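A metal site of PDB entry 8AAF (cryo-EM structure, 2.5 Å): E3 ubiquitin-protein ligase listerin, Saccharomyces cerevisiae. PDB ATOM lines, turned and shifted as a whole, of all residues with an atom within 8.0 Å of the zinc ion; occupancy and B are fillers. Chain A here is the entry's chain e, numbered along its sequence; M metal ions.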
ATOM      1  N   THR A1526     -16.953 -23.837  -1.755  1.00  0.00           N
ATOM      2  CA  THR A1526     -17.598 -22.580  -1.378  1.00  0.00           C
ATOM      3  C   THR A1526     -16.549 -21.514  -1.145  1.00  0.00           C
ATOM      4  O   THR A1526     -15.572 -21.745  -0.438  1.00  0.00           O
ATOM      5  CB  THR A1526     -18.441 -22.743  -0.084  1.00  0.00           C
ATOM      6  OG1 THR A1526     -17.665 -23.410   0.913  1.00  0.00           O
ATOM      7  CG2 THR A1526     -19.701 -23.538  -0.365  1.00  0.00           C
ATOM      8  N   CYS A1527     -16.747 -20.349  -1.742  1.00  0.00           N
ATOM      9  CA  CYS A1527     -15.816 -19.243  -1.548  1.00  0.00           C
ATOM     10  C   CYS A1527     -15.889 -18.770  -0.103  1.00  0.00           C
ATOM     11  O   CYS A1527     -16.973 -18.666   0.460  1.00  0.00           O
ATOM     12  CB  CYS A1527     -16.182 -18.118  -2.505  1.00  0.00           C
ATOM     13  SG  CYS A1527     -15.207 -16.609  -2.416  1.00  0.00           S
ATOM     14  N   PRO A1528     -14.735 -18.502   0.517  1.00  0.00           N
ATOM     15  CA  PRO A1528     -14.826 -17.965   1.874  1.00  0.00           C
ATOM     16  C   PRO A1528     -15.484 -16.593   1.853  1.00  0.00           C
ATOM     17  O   PRO A1528     -16.333 -16.310   2.706  1.00  0.00           O
ATOM     18  CB  PRO A1528     -13.358 -17.820   2.294  1.00  0.00           C
ATOM     19  CG  PRO A1528     -12.618 -18.772   1.416  1.00  0.00           C
ATOM     20  CD  PRO A1528     -13.345 -18.775   0.115  1.00  0.00           C
ATOM     21  N   THR A1529     -15.102 -15.755   0.911  1.00  0.00           N
ATOM     22  CA  THR A1529     -15.662 -14.406   0.806  1.00  0.00           C
ATOM     23  C   THR A1529     -17.144 -14.371   0.457  1.00  0.00           C
ATOM     24  O   THR A1529     -17.898 -13.589   1.036  1.00  0.00           O
ATOM     25  CB  THR A1529     -14.895 -13.574  -0.215  1.00  0.00           C
ATOM     26  OG1 THR A1529     -13.504 -13.918  -0.149  1.00  0.00           O
ATOM     27  CG2 THR A1529     -15.069 -12.088   0.061  1.00  0.00           C
ATOM     28  N   CYS A1530     -17.572 -15.210  -0.467  1.00  0.00           N
ATOM     29  CA  CYS A1530     -18.967 -15.168  -0.899  1.00  0.00           C
ATOM     30  C   CYS A1530     -19.687 -16.502  -0.763  1.00  0.00           C
ATOM     31  O   CYS A1530     -19.082 -17.559  -0.946  1.00  0.00           O
ATOM     32  CB  CYS A1530     -19.100 -14.592  -2.326  1.00  0.00           C
ATOM     33  SG  CYS A1530     -18.438 -15.595  -3.673  1.00  0.00           S
ATOM     34  N   LYS A1531     -20.976 -16.473  -0.489  1.00  0.00           N
ATOM     35  CA  LYS A1531     -21.736 -17.700  -0.261  1.00  0.00           C
ATOM     36  C   LYS A1531     -21.903 -18.573  -1.492  1.00  0.00           C
ATOM     37  O   LYS A1531     -22.303 -19.726  -1.383  1.00  0.00           O
ATOM     38  CB  LYS A1531     -23.115 -17.376   0.335  1.00  0.00           C
ATOM     39  CG  LYS A1531     -23.053 -16.666   1.678  1.00  0.00           C
ATOM     40  CD  LYS A1531     -24.445 -16.370   2.211  1.00  0.00           C
ATOM     41  CE  LYS A1531     -24.381 -15.643   3.537  1.00  0.00           C
ATOM     42  NZ  LYS A1531     -25.743 -15.314   4.066  1.00  0.00           N
ATOM     43  N   ASN A1532     -21.618 -18.030  -2.667  1.00  0.00           N
ATOM     44  CA  ASN A1532     -21.848 -18.781  -3.897  1.00  0.00           C
ATOM     45  C   ASN A1532     -21.105 -20.097  -3.947  1.00  0.00           C
ATOM     46  O   ASN A1532     -19.950 -20.191  -3.509  1.00  0.00           O
ATOM     47  CB  ASN A1532     -21.475 -17.913  -5.097  1.00  0.00           C
ATOM     48  CG  ASN A1532     -22.230 -16.608  -5.128  1.00  0.00           C
ATOM     49  OD1 ASN A1532     -21.728 -15.578  -4.681  1.00  0.00           O
ATOM     50  ND2 ASN A1532     -23.455 -16.642  -5.651  1.00  0.00           N
ATOM     51  N   PHE A1534     -19.410 -23.268  -5.990  1.00  0.00           N
ATOM     52  CA  PHE A1534     -18.803 -23.544  -7.280  1.00  0.00           C
ATOM     53  C   PHE A1534     -18.465 -25.010  -7.404  1.00  0.00           C
ATOM     54  O   PHE A1534     -18.027 -25.626  -6.446  1.00  0.00           O
ATOM     55  CB  PHE A1534     -17.499 -22.763  -7.439  1.00  0.00           C
ATOM     56  CG  PHE A1534     -17.626 -21.284  -7.206  1.00  0.00           C
ATOM     57  CD1 PHE A1534     -18.014 -20.437  -8.215  1.00  0.00           C
ATOM     58  CD2 PHE A1534     -17.332 -20.742  -5.964  1.00  0.00           C
ATOM     59  CE1 PHE A1534     -18.126 -19.074  -8.003  1.00  0.00           C
ATOM     60  CE2 PHE A1534     -17.450 -19.387  -5.738  1.00  0.00           C
ATOM     61  CZ  PHE A1534     -17.849 -18.551  -6.763  1.00  0.00           C
ATOM     62  N   LEU A1539     -14.308 -24.259 -10.784  1.00  0.00           N
ATOM     63  CA  LEU A1539     -13.474 -23.325 -10.033  1.00  0.00           C
ATOM     64  C   LEU A1539     -12.008 -23.485 -10.398  1.00  0.00           C
ATOM     65  O   LEU A1539     -11.309 -22.499 -10.592  1.00  0.00           O
ATOM     66  CB  LEU A1539     -13.649 -23.559  -8.533  1.00  0.00           C
ATOM     67  CG  LEU A1539     -13.100 -22.479  -7.615  1.00  0.00           C
ATOM     68  CD1 LEU A1539     -13.786 -21.160  -7.914  1.00  0.00           C
ATOM     69  CD2 LEU A1539     -13.293 -22.872  -6.160  1.00  0.00           C
ATOM     70  N   THR A1550      -8.169 -17.089  -7.523  1.00  0.00           N
ATOM     71  CA  THR A1550      -9.043 -15.918  -7.569  1.00  0.00           C
ATOM     72  C   THR A1550     -10.480 -16.316  -7.839  1.00  0.00           C
ATOM     73  O   THR A1550     -10.767 -16.999  -8.812  1.00  0.00           O
ATOM     74  CB  THR A1550      -8.590 -14.929  -8.649  1.00  0.00           C
ATOM     75  OG1 THR A1550      -8.364 -15.627  -9.878  1.00  0.00           O
ATOM     76  CG2 THR A1550      -7.305 -14.226  -8.239  1.00  0.00           C
ATOM     77  N   CYS A1551     -11.397 -15.870  -6.990  1.00  0.00           N
ATOM     78  CA  CYS A1551     -12.813 -16.183  -7.177  1.00  0.00           C
ATOM     79  C   CYS A1551     -13.350 -15.521  -8.436  1.00  0.00           C
ATOM     80  O   CYS A1551     -13.050 -14.369  -8.720  1.00  0.00           O
ATOM     81  CB  CYS A1551     -13.590 -15.708  -5.962  1.00  0.00           C
ATOM     82  SG  CYS A1551     -15.379 -15.925  -6.019  1.00  0.00           S
ATOM     83  N   PRO A1552     -14.138 -16.269  -9.230  1.00  0.00           N
ATOM     84  CA  PRO A1552     -14.726 -15.598 -10.404  1.00  0.00           C
ATOM     85  C   PRO A1552     -15.717 -14.500 -10.038  1.00  0.00           C
ATOM     86  O   PRO A1552     -15.648 -13.407 -10.604  1.00  0.00           O
ATOM     87  CB  PRO A1552     -15.490 -16.735 -11.103  1.00  0.00           C
ATOM     88  CG  PRO A1552     -14.989 -18.002 -10.509  1.00  0.00           C
ATOM     89  CD  PRO A1552     -14.517 -17.679  -9.131  1.00  0.00           C
ATOM     90  N   LEU A1553     -16.615 -14.779  -9.103  1.00  0.00           N
ATOM     91  CA  LEU A1553     -17.618 -13.792  -8.715  1.00  0.00           C
ATOM     92  C   LEU A1553     -17.078 -12.578  -7.986  1.00  0.00           C
ATOM     93  O   LEU A1553     -17.531 -11.457  -8.215  1.00  0.00           O
ATOM     94  CB  LEU A1553     -18.757 -14.428  -7.926  1.00  0.00           C
ATOM     95  CG  LEU A1553     -19.776 -15.172  -8.790  1.00  0.00           C
ATOM     96  CD1 LEU A1553     -21.148 -15.094  -8.154  1.00  0.00           C
ATOM     97  CD2 LEU A1553     -19.828 -14.565 -10.192  1.00  0.00           C
ATOM     98  N   CYS A1554     -16.116 -12.783  -7.094  1.00  0.00           N
ATOM     99  CA  CYS A1554     -15.621 -11.675  -6.290  1.00  0.00           C
ATOM    100  C   CYS A1554     -14.104 -11.525  -6.359  1.00  0.00           C
ATOM    101  O   CYS A1554     -13.392 -12.478  -6.633  1.00  0.00           O
ATOM    102  CB  CYS A1554     -16.074 -11.810  -4.830  1.00  0.00           C
ATOM    103  SG  CYS A1554     -15.149 -13.015  -3.851  1.00  0.00           S
ATOM    104  N   ARG A1555     -13.620 -10.315  -6.120  1.00  0.00           N
ATOM    105  CA  ARG A1555     -12.183 -10.065  -6.200  1.00  0.00           C
ATOM    106  C   ARG A1555     -11.371 -10.864  -5.198  1.00  0.00           C
ATOM    107  O   ARG A1555     -10.268 -11.315  -5.510  1.00  0.00           O
ATOM    108  CB  ARG A1555     -11.881  -8.564  -6.050  1.00  0.00           C
ATOM    109  CG  ARG A1555     -11.995  -7.767  -7.327  1.00  0.00           C
ATOM    110  CD  ARG A1555     -13.447  -7.447  -7.680  1.00  0.00           C
ATOM    111  NE  ARG A1555     -13.598  -7.125  -9.094  1.00  0.00           N
ATOM    112  CZ  ARG A1555     -13.937  -8.010 -10.028  1.00  0.00           C
ATOM    113  NH1 ARG A1555     -14.149  -9.272  -9.708  1.00  0.00           N
ATOM    114  NH2 ARG A1555     -14.055  -7.632 -11.294  1.00  0.00           N
ATOM    115  N   SER A1556     -11.894 -11.037  -3.987  1.00  0.00           N
ATOM    116  CA  SER A1556     -11.116 -11.707  -2.935  1.00  0.00           C
ATOM    117  C   SER A1556     -10.726 -13.145  -3.234  1.00  0.00           C
ATOM    118  O   SER A1556     -11.496 -13.896  -3.835  1.00  0.00           O
ATOM    119  CB  SER A1556     -11.835 -11.609  -1.600  1.00  0.00           C
ATOM    120  OG  SER A1556     -11.108 -12.276  -0.577  1.00  0.00           O
ATOM    121  N   GLU A1557      -9.527 -13.535  -2.815  1.00  0.00           N
ATOM    122  CA  GLU A1557      -9.009 -14.869  -3.099  1.00  0.00           C
ATOM    123  C   GLU A1557      -9.637 -16.052  -2.361  1.00  0.00           C
ATOM    124  O   GLU A1557     -10.178 -15.897  -1.265  1.00  0.00           O
ATOM    125  CB  GLU A1557      -7.506 -14.893  -2.842  1.00  0.00           C
ATOM    126  N   ILE A1558      -9.571 -17.235  -2.972  1.00  0.00           N
ATOM    127  CA  ILE A1558     -10.069 -18.441  -2.321  1.00  0.00           C
ATOM    128  C   ILE A1558      -8.868 -19.318  -2.024  1.00  0.00           C
ATOM    129  O   ILE A1558      -8.064 -19.586  -2.913  1.00  0.00           O
ATOM    130  CB  ILE A1558     -10.985 -19.246  -3.255  1.00  0.00           C
ATOM    131  CG1 ILE A1558     -12.158 -18.400  -3.735  1.00  0.00           C
ATOM    132  CG2 ILE A1558     -11.488 -20.514  -2.579  1.00  0.00           C
ATOM    133  CD1 ILE A1558     -13.136 -19.173  -4.602  1.00  0.00           C
HETATM  134 ZN    ZN M   1     -16.159 -15.127  -3.962  1.00  0.00          ZN
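The backbone NH of Leu 1553 sits close to the side-chain sulfur of Cys 1551 (3.5 Å). The side-chain sulfur (SG) of Cys 1527 sits close to the backbone NH (N) of Thr 1529, 3.4 Å away. The side-chain amide oxygen of Asn 1532 lies close to the side-chain sulfur of Cys 1530 (3.4 Å). The backbone carbonyl oxygen (O) of Ser 1556 sits close to the side-chain sulfur (SG) of Cys 1554.
SG of Cys 1551 is bound to the zinc ion (2.3 Å). SG of Cys 1527 is bound to the zinc ion, 2.3 Å away. The zinc ion is bound by the side-chain sulfur (SG) of Cys 1530, 2.3 Å away. The side-chain sulfur (SG) of Cys 1554 binds the zinc ion (2.3 Å). The zinc ion has four donor atoms within binding distance.
The nearest printed residue that does not touch the zinc ion is Thr 1529 (4.2 Å).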
